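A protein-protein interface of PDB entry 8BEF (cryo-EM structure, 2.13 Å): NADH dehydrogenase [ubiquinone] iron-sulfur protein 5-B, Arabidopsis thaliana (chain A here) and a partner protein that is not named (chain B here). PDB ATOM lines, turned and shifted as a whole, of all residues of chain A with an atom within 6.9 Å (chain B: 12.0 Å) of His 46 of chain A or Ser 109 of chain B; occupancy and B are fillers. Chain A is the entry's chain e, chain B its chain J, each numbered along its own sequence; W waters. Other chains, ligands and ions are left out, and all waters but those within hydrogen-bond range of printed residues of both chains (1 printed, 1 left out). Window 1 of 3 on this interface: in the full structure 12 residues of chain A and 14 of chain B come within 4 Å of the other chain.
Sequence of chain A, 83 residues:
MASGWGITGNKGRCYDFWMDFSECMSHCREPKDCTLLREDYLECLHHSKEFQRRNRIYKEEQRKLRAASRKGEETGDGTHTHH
The side-chain carboxylate (OE1) of Glu 43 of chain A is in hydrogen-bond range of the backbone NH (N) of Ser 48 of chain A (3.3 Å).
The side-chain sulfur (SG) of Cys 14 of chain A is disulfide-bonded to the side-chain sulfur (SG) of Cys 44 of chain A, at 2.1 Å.
Of the 12 printed residues of chain A, 3 touch a printed residue of chain B.
Hydrophobic or aromatic side chains of chain A within 4 Å of the printed part of chain B: His 46 and Phe 51.
Along chain A the printed residues that touch a printed residue of chain B span positions 46 to 51.
Among the printed residues, 6 pairs touch across the chains.
Among the printed residues, no Asp or Glu carboxylate lies within 4 Å of a Lys or Arg side-chain nitrogen of the other chain.
Of chain B, only Glu 108 (3.3 Å) and Ser 109 (3.6 Å) come within 4 Å of His 46 of chain A.
Ser 109 of chain B touches one residue of chain A.
No residue of chain B comes within 4 Å of Leu 42 of chain A.
No residue of chain B comes within 4 Å of Glu 43 of chain A.
No residue of chain B comes within 4 Å of Leu 45 of chain A.
His 47 of chain A touches none of the printed residues of chain B.
Ser 48 of chain A touches two residues of chain B.
Printed residues of chain A within 4 Å of Leu 112 of chain B: Phe 51.
Printed residues of chain A within 4 Å of Ile 110 of chain B: Ser 48 and Phe 51.
Of the printed residues of chain A, Glu 108 of chain B touches His 46 and Ser 48.
Glu 100 of chain B touches none of the printed residues of chain A.
Cys 14 of chain A touches none of the printed residues of chain B.
The nearest residue of chain B that does not touch His 46 of chain A is Ile 110 of chain B (5.0 Å).
The nearest residue of chain A that does not touch Ser 109 of chain B is Ser 48 of chain A (5.3 Å).
The nearest printed residue of chain B that does not touch Phe 51 of chain A is Pro 111 of chain B (4.3 Å).
Water W1 lies within hydrogen-bond range of the side-chain hydroxyl (OG) of Ser 109 of chain B and a ring nitrogen (ND1) of His 46 of chain A.
Among the printed residues, pairs that only touch across the chains: His 46 of chain A with Glu 108 of chain B, His 46 of chain A with Ser 109 of chain B, Ser 48 of chain A with Glu 108 of chain B, Ser 48 of chain A with Ile 110 of chain B, Phe 51 of chain A with Ile 110 of chain B and Phe 51 of chain A with Leu 112 of chain B.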
ATOM      1  N   ARG A  13      -6.503  18.967 -13.322  1.00  0.00           N
ATOM      2  CA  ARG A  13      -6.106  18.137 -12.186  1.00  0.00           C
ATOM      3  C   ARG A  13      -5.158  18.875 -11.245  1.00  0.00           C
ATOM      4  O   ARG A  13      -5.287  18.775 -10.021  1.00  0.00           O
ATOM      5  CB  ARG A  13      -5.461  16.841 -12.685  1.00  0.00           C
ATOM      6  CG  ARG A  13      -4.532  16.177 -11.668  1.00  0.00           C
ATOM      7  CD  ARG A  13      -3.964  14.855 -12.166  1.00  0.00           C
ATOM      8  NE  ARG A  13      -2.608  14.989 -12.685  1.00  0.00           N
ATOM      9  CZ  ARG A  13      -2.295  14.897 -13.971  1.00  0.00           C
ATOM     10  NH1 ARG A  13      -3.217  14.660 -14.889  1.00  0.00           N
ATOM     11  NH2 ARG A  13      -1.027  15.041 -14.343  1.00  0.00           N
ATOM     12  N   CYS A  14      -4.166  19.578 -11.805  1.00  0.00           N
ATOM     13  CA  CYS A  14      -3.068  20.252 -11.080  1.00  0.00           C
ATOM     14  C   CYS A  14      -3.255  21.776 -10.863  1.00  0.00           C
ATOM     15  O   CYS A  14      -2.383  22.371 -10.363  1.00  0.00           O
ATOM     16  CB  CYS A  14      -1.782  19.980 -11.845  1.00  0.00           C
ATOM     17  SG  CYS A  14      -1.456  18.217 -12.057  1.00  0.00           S
ATOM     18  N   TYR A  41       3.145  21.015  -7.015  1.00  0.00           N
ATOM     19  CA  TYR A  41       2.662  21.267  -8.408  1.00  0.00           C
ATOM     20  C   TYR A  41       3.386  20.345  -9.411  1.00  0.00           C
ATOM     21  O   TYR A  41       2.706  19.641 -10.089  1.00  0.00           O
ATOM     22  CB  TYR A  41       2.766  22.759  -8.744  1.00  0.00           C
ATOM     23  CG  TYR A  41       2.508  23.035 -10.209  1.00  0.00           C
ATOM     24  CD1 TYR A  41       1.242  22.890 -10.739  1.00  0.00           C
ATOM     25  CD2 TYR A  41       3.540  23.362 -11.074  1.00  0.00           C
ATOM     26  CE1 TYR A  41       0.990  23.117 -12.081  1.00  0.00           C
ATOM     27  CE2 TYR A  41       3.314  23.592 -12.421  1.00  0.00           C
ATOM     28  CZ  TYR A  41       2.028  23.466 -12.925  1.00  0.00           C
ATOM     29  OH  TYR A  41       1.761  23.683 -14.237  1.00  0.00           O
ATOM     30  N   LEU A  42       4.713  20.305  -9.368  1.00  0.00           N
ATOM     31  CA  LEU A  42       5.437  19.492 -10.343  1.00  0.00           C
ATOM     32  C   LEU A  42       5.198  17.997 -10.129  1.00  0.00           C
ATOM     33  O   LEU A  42       5.157  17.232 -11.104  1.00  0.00           O
ATOM     34  CB  LEU A  42       6.927  19.825 -10.300  1.00  0.00           C
ATOM     35  CG  LEU A  42       7.277  21.264 -10.704  1.00  0.00           C
ATOM     36  CD1 LEU A  42       8.774  21.504 -10.630  1.00  0.00           C
ATOM     37  CD2 LEU A  42       6.751  21.601 -12.096  1.00  0.00           C
ATOM     38  N   GLU A  43       5.025  17.566  -8.875  1.00  0.00           N
ATOM     39  CA  GLU A  43       4.656  16.182  -8.597  1.00  0.00           C
ATOM     40  C   GLU A  43       3.290  15.849  -9.176  1.00  0.00           C
ATOM     41  O   GLU A  43       3.085  14.756  -9.712  1.00  0.00           O
ATOM     42  CB  GLU A  43       4.670  15.936  -7.086  1.00  0.00           C
ATOM     43  CG  GLU A  43       4.275  14.526  -6.643  1.00  0.00           C
ATOM     44  CD  GLU A  43       5.167  13.432  -7.212  1.00  0.00           C
ATOM     45  OE1 GLU A  43       6.360  13.690  -7.470  1.00  0.00           O
ATOM     46  OE2 GLU A  43       4.676  12.300  -7.388  1.00  0.00           O
ATOM     47  N   CYS A  44       2.334  16.773  -9.062  1.00  0.00           N
ATOM     48  CA  CYS A  44       1.046  16.557  -9.710  1.00  0.00           C
ATOM     49  C   CYS A  44       1.211  16.444 -11.220  1.00  0.00           C
ATOM     50  O   CYS A  44       0.533  15.637 -11.868  1.00  0.00           O
ATOM     51  CB  CYS A  44       0.073  17.682  -9.361  1.00  0.00           C
ATOM     52  SG  CYS A  44      -1.577  17.484 -10.075  1.00  0.00           S
ATOM     53  N   LEU A  45       2.100  17.135 -11.861  1.00  0.00           N
ATOM     54  CA  LEU A  45       2.245  17.062 -13.343  1.00  0.00           C
ATOM     55  C   LEU A  45       2.864  15.722 -13.727  1.00  0.00           C
ATOM     56  O   LEU A  45       2.372  15.124 -14.628  1.00  0.00           O
ATOM     57  CB  LEU A  45       3.191  18.119 -13.893  1.00  0.00           C
ATOM     58  CG  LEU A  45       2.790  19.590 -13.763  1.00  0.00           C
ATOM     59  CD1 LEU A  45       3.796  20.469 -14.483  1.00  0.00           C
ATOM     60  CD2 LEU A  45       1.397  19.862 -14.280  1.00  0.00           C
ATOM     61  N   HIS A  46       3.903  15.321 -12.990  1.00  0.00           N
ATOM     62  CA  HIS A  46       4.631  14.165 -13.506  1.00  0.00           C
ATOM     63  C   HIS A  46       4.608  12.917 -12.627  1.00  0.00           C
ATOM     64  O   HIS A  46       5.037  11.859 -13.098  1.00  0.00           O
ATOM     65  CB  HIS A  46       6.095  14.538 -13.786  1.00  0.00           C
ATOM     66  CG  HIS A  46       6.263  15.857 -14.472  1.00  0.00           C
ATOM     67  ND1 HIS A  46       5.898  16.066 -15.784  1.00  0.00           N
ATOM     68  CD2 HIS A  46       6.768  17.033 -14.030  1.00  0.00           C
ATOM     69  CE1 HIS A  46       6.164  17.315 -16.120  1.00  0.00           C
ATOM     70  NE2 HIS A  46       6.693  17.924 -15.074  1.00  0.00           N
ATOM     71  N   HIS A  47       4.134  12.999 -11.382  1.00  0.00           N
ATOM     72  CA  HIS A  47       4.070  11.845 -10.475  1.00  0.00           C
ATOM     73  C   HIS A  47       5.428  11.166 -10.301  1.00  0.00           C
ATOM     74  O   HIS A  47       5.503   9.946 -10.153  1.00  0.00           O
ATOM     75  CB  HIS A  47       3.041  10.809 -10.940  1.00  0.00           C
ATOM     76  CG  HIS A  47       1.739  11.395 -11.386  1.00  0.00           C
ATOM     77  ND1 HIS A  47       0.875  12.033 -10.524  1.00  0.00           N
ATOM     78  CD2 HIS A  47       1.146  11.425 -12.603  1.00  0.00           C
ATOM     79  CE1 HIS A  47      -0.191  12.435 -11.190  1.00  0.00           C
ATOM     80  NE2 HIS A  47      -0.051  12.079 -12.453  1.00  0.00           N
ATOM     81  N   SER A  48       6.511  11.942 -10.314  1.00  0.00           N
ATOM     82  CA  SER A  48       7.842  11.345 -10.317  1.00  0.00           C
ATOM     83  C   SER A  48       8.137  10.625  -9.004  1.00  0.00           C
ATOM     84  O   SER A  48       8.575   9.469  -9.005  1.00  0.00           O
ATOM     85  CB  SER A  48       8.894  12.416 -10.601  1.00  0.00           C
ATOM     86  OG  SER A  48      10.149  12.062 -10.052  1.00  0.00           O
ATOM     87  N   LYS A  49       7.894  11.286  -7.870  1.00  0.00           N
ATOM     88  CA  LYS A  49       8.222  10.671  -6.587  1.00  0.00           C
ATOM     89  C   LYS A  49       7.290   9.508  -6.266  1.00  0.00           C
ATOM     90  O   LYS A  49       7.728   8.491  -5.714  1.00  0.00           O
ATOM     91  CB  LYS A  49       8.201  11.717  -5.473  1.00  0.00           C
ATOM     92  CG  LYS A  49       9.303  12.757  -5.604  1.00  0.00           C
ATOM     93  CD  LYS A  49       9.148  13.919  -4.629  1.00  0.00           C
ATOM     94  CE  LYS A  49       7.710  14.316  -4.412  1.00  0.00           C
ATOM     95  NZ  LYS A  49       7.267  15.244  -5.474  1.00  0.00           N
ATOM     96  N   PHE A  51       5.828   7.426  -8.434  1.00  0.00           N
ATOM     97  CA  PHE A  51       6.240   6.279  -9.232  1.00  0.00           C
ATOM     98  C   PHE A  51       7.591   5.744  -8.771  1.00  0.00           C
ATOM     99  O   PHE A  51       7.817   4.533  -8.788  1.00  0.00           O
ATOM    100  CB  PHE A  51       6.271   6.656 -10.715  1.00  0.00           C
ATOM    101  CG  PHE A  51       4.905   6.898 -11.307  1.00  0.00           C
ATOM    102  CD1 PHE A  51       3.762   6.552 -10.608  1.00  0.00           C
ATOM    103  CD2 PHE A  51       4.766   7.467 -12.562  1.00  0.00           C
ATOM    104  CE1 PHE A  51       2.511   6.772 -11.141  1.00  0.00           C
ATOM    105  CE2 PHE A  51       3.513   7.690 -13.104  1.00  0.00           C
ATOM    106  CZ  PHE A  51       2.385   7.343 -12.394  1.00  0.00           C
ATOM    107  N   GLU B 100      19.996  11.725 -26.174  1.00  0.00           N
ATOM    108  CA  GLU B 100      19.506  12.863 -25.417  1.00  0.00           C
ATOM    109  C   GLU B 100      17.993  12.947 -25.393  1.00  0.00           C
ATOM    110  O   GLU B 100      17.406  13.290 -24.363  1.00  0.00           O
ATOM    111  CB  GLU B 100      20.034  14.151 -26.036  1.00  0.00           C
ATOM    112  CG  GLU B 100      19.707  15.342 -25.218  1.00  0.00           C
ATOM    113  CD  GLU B 100      20.658  15.479 -24.080  1.00  0.00           C
ATOM    114  OE1 GLU B 100      21.873  15.355 -24.321  1.00  0.00           O
ATOM    115  OE2 GLU B 100      20.185  15.669 -22.941  1.00  0.00           O
ATOM    116  N   MET B 101      17.363  12.632 -26.495  1.00  0.00           N
ATOM    117  CA  MET B 101      16.065  13.181 -26.814  1.00  0.00           C
ATOM    118  C   MET B 101      14.947  12.144 -26.765  1.00  0.00           C
ATOM    119  O   MET B 101      13.782  12.515 -26.614  1.00  0.00           O
ATOM    120  CB  MET B 101      16.169  13.870 -28.185  1.00  0.00           C
ATOM    121  CG  MET B 101      14.951  14.018 -28.953  1.00  0.00           C
ATOM    122  SD  MET B 101      14.436  15.743 -28.838  1.00  0.00           S
ATOM    123  CE  MET B 101      15.692  16.624 -29.777  1.00  0.00           C
ATOM    124  N   PHE B 102      15.271  10.854 -26.884  1.00  0.00           N
ATOM    125  CA  PHE B 102      14.318   9.792 -26.561  1.00  0.00           C
ATOM    126  C   PHE B 102      14.175   9.571 -25.062  1.00  0.00           C
ATOM    127  O   PHE B 102      13.195   8.961 -24.633  1.00  0.00           O
ATOM    128  CB  PHE B 102      14.733   8.470 -27.212  1.00  0.00           C
ATOM    129  CG  PHE B 102      14.534   8.427 -28.692  1.00  0.00           C
ATOM    130  CD1 PHE B 102      15.333   9.186 -29.531  1.00  0.00           C
ATOM    131  CD2 PHE B 102      13.569   7.612 -29.253  1.00  0.00           C
ATOM    132  CE1 PHE B 102      15.152   9.143 -30.896  1.00  0.00           C
ATOM    133  CE2 PHE B 102      13.389   7.564 -30.617  1.00  0.00           C
ATOM    134  CZ  PHE B 102      14.181   8.329 -31.436  1.00  0.00           C
ATOM    135  N   PHE B 103      15.131  10.052 -24.263  1.00  0.00           N
ATOM    136  CA  PHE B 103      15.168   9.796 -22.826  1.00  0.00           C
ATOM    137  C   PHE B 103      15.040  11.069 -22.004  1.00  0.00           C
ATOM    138  O   PHE B 103      15.315  11.046 -20.800  1.00  0.00           O
ATOM    139  CB  PHE B 103      16.462   9.061 -22.457  1.00  0.00           C
ATOM    140  CG  PHE B 103      16.731   7.851 -23.306  1.00  0.00           C
ATOM    141  CD1 PHE B 103      15.979   6.699 -23.150  1.00  0.00           C
ATOM    142  CD2 PHE B 103      17.719   7.874 -24.276  1.00  0.00           C
ATOM    143  CE1 PHE B 103      16.216   5.585 -23.936  1.00  0.00           C
ATOM    144  CE2 PHE B 103      17.960   6.765 -25.065  1.00  0.00           C
ATOM    145  CZ  PHE B 103      17.205   5.619 -24.896  1.00  0.00           C
ATOM    146  N   ILE B 104      14.630  12.178 -22.624  1.00  0.00           N
ATOM    147  CA  ILE B 104      14.559  13.460 -21.930  1.00  0.00           C
ATOM    148  C   ILE B 104      13.496  13.436 -20.838  1.00  0.00           C
ATOM    149  O   ILE B 104      13.659  14.073 -19.792  1.00  0.00           O
ATOM    150  CB  ILE B 104      14.317  14.584 -22.957  1.00  0.00           C
ATOM    151  CG1 ILE B 104      14.095  15.934 -22.282  1.00  0.00           C
ATOM    152  CG2 ILE B 104      13.155  14.252 -23.837  1.00  0.00           C
ATOM    153  CD1 ILE B 104      14.566  17.098 -23.113  1.00  0.00           C
ATOM    154  N   LEU B 105      12.404  12.701 -21.053  1.00  0.00           N
ATOM    155  CA  LEU B 105      11.331  12.620 -20.072  1.00  0.00           C
ATOM    156  C   LEU B 105      11.635  11.666 -18.922  1.00  0.00           C
ATOM    157  O   LEU B 105      10.910  11.685 -17.922  1.00  0.00           O
ATOM    158  CB  LEU B 105      10.026  12.182 -20.748  1.00  0.00           C
ATOM    159  CG  LEU B 105       9.453  13.004 -21.905  1.00  0.00           C
ATOM    160  CD1 LEU B 105       7.983  12.670 -22.119  1.00  0.00           C
ATOM    161  CD2 LEU B 105       9.625  14.489 -21.665  1.00  0.00           C
ATOM    162  N   ASP B 106      12.680  10.841 -19.035  1.00  0.00           N
ATOM    163  CA  ASP B 106      12.880   9.760 -18.074  1.00  0.00           C
ATOM    164  C   ASP B 106      13.135  10.283 -16.664  1.00  0.00           C
ATOM    165  O   ASP B 106      12.631   9.717 -15.690  1.00  0.00           O
ATOM    166  CB  ASP B 106      14.024   8.858 -18.534  1.00  0.00           C
ATOM    167  CG  ASP B 106      13.672   8.074 -19.787  1.00  0.00           C
ATOM    168  OD1 ASP B 106      12.940   8.617 -20.640  1.00  0.00           O
ATOM    169  OD2 ASP B 106      14.117   6.917 -19.915  1.00  0.00           O
ATOM    170  N   ASN B 107      13.916  11.355 -16.530  1.00  0.00           N
ATOM    171  CA  ASN B 107      14.215  11.874 -15.199  1.00  0.00           C
ATOM    172  C   ASN B 107      13.035  12.641 -14.616  1.00  0.00           C
ATOM    173  O   ASN B 107      12.807  12.605 -13.402  1.00  0.00           O
ATOM    174  CB  ASN B 107      15.455  12.763 -15.247  1.00  0.00           C
ATOM    175  CG  ASN B 107      16.737  11.969 -15.166  1.00  0.00           C
ATOM    176  OD1 ASN B 107      16.779  10.797 -15.539  1.00  0.00           O
ATOM    177  ND2 ASN B 107      17.795  12.604 -14.678  1.00  0.00           N
ATOM    178  N   GLU B 108      12.278  13.336 -15.462  1.00  0.00           N
ATOM    179  CA  GLU B 108      11.121  14.078 -14.983  1.00  0.00           C
ATOM    180  C   GLU B 108       9.900  13.178 -14.848  1.00  0.00           C
ATOM    181  O   GLU B 108       9.174  13.259 -13.852  1.00  0.00           O
ATOM    182  CB  GLU B 108      10.818  15.243 -15.922  1.00  0.00           C
ATOM    183  CG  GLU B 108       9.912  16.299 -15.323  1.00  0.00           C
ATOM    184  CD  GLU B 108      10.625  17.152 -14.293  1.00  0.00           C
ATOM    185  OE1 GLU B 108      10.703  16.730 -13.120  1.00  0.00           O
ATOM    186  OE2 GLU B 108      11.111  18.243 -14.656  1.00  0.00           O
ATOM    187  N   SER B 109       9.663  12.320 -15.834  1.00  0.00           N
ATOM    188  CA  SER B 109       8.504  11.433 -15.860  1.00  0.00           C
ATOM    189  C   SER B 109       9.016  10.000 -15.768  1.00  0.00           C
ATOM    190  O   SER B 109       9.227   9.331 -16.782  1.00  0.00           O
ATOM    191  CB  SER B 109       7.681  11.664 -17.114  1.00  0.00           C
ATOM    192  OG  SER B 109       7.064  12.939 -17.077  1.00  0.00           O
ATOM    193  N   ILE B 110       9.214   9.536 -14.543  1.00  0.00           N
ATOM    194  CA  ILE B 110       9.724   8.184 -14.309  1.00  0.00           C
ATOM    195  C   ILE B 110       8.588   7.187 -14.523  1.00  0.00           C
ATOM    196  O   ILE B 110       7.516   7.345 -13.924  1.00  0.00           O
ATOM    197  CB  ILE B 110      10.300   8.068 -12.903  1.00  0.00           C
ATOM    198  CG1 ILE B 110      11.607   8.854 -12.806  1.00  0.00           C
ATOM    199  CG2 ILE B 110      10.529   6.610 -12.535  1.00  0.00           C
ATOM    200  CD1 ILE B 110      11.943   9.300 -11.424  1.00  0.00           C
ATOM    201  N   PRO B 111       8.777   6.171 -15.357  1.00  0.00           N
ATOM    202  CA  PRO B 111       7.691   5.221 -15.615  1.00  0.00           C
ATOM    203  C   PRO B 111       7.353   4.384 -14.392  1.00  0.00           C
ATOM    204  O   PRO B 111       8.201   4.091 -13.548  1.00  0.00           O
ATOM    205  CB  PRO B 111       8.244   4.350 -16.747  1.00  0.00           C
ATOM    206  CG  PRO B 111       9.712   4.452 -16.617  1.00  0.00           C
ATOM    207  CD  PRO B 111       9.998   5.836 -16.105  1.00  0.00           C
ATOM    208  N   LEU B 112       6.084   4.000 -14.312  1.00  0.00           N
ATOM    209  CA  LEU B 112       5.629   3.055 -13.302  1.00  0.00           C
ATOM    210  C   LEU B 112       5.857   1.638 -13.813  1.00  0.00           C
ATOM    211  O   LEU B 112       5.243   1.225 -14.801  1.00  0.00           O
ATOM    212  CB  LEU B 112       4.155   3.292 -12.988  1.00  0.00           C
ATOM    213  CG  LEU B 112       3.540   2.504 -11.834  1.00  0.00           C
ATOM    214  CD1 LEU B 112       4.114   2.953 -10.497  1.00  0.00           C
ATOM    215  CD2 LEU B 112       2.028   2.638 -11.852  1.00  0.00           C
ATOM    216  N   LEU B 113       6.740   0.899 -13.152  1.00  0.00           N
ATOM    217  CA  LEU B 113       7.004  -0.475 -13.561  1.00  0.00           C
ATOM    218  C   LEU B 113       5.783  -1.343 -13.275  1.00  0.00           C
ATOM    219  O   LEU B 113       5.277  -1.340 -12.147  1.00  0.00           O
ATOM    220  CB  LEU B 113       8.234  -1.027 -12.843  1.00  0.00           C
ATOM    221  CG  LEU B 113       9.487  -0.158 -12.960  1.00  0.00           C
ATOM    222  CD1 LEU B 113      10.653  -0.760 -12.204  1.00  0.00           C
ATOM    223  CD2 LEU B 113       9.845   0.050 -14.424  1.00  0.00           C
HETATM  224  O   HOH W   1       4.668  13.773 -16.960  1.00  0.00           O
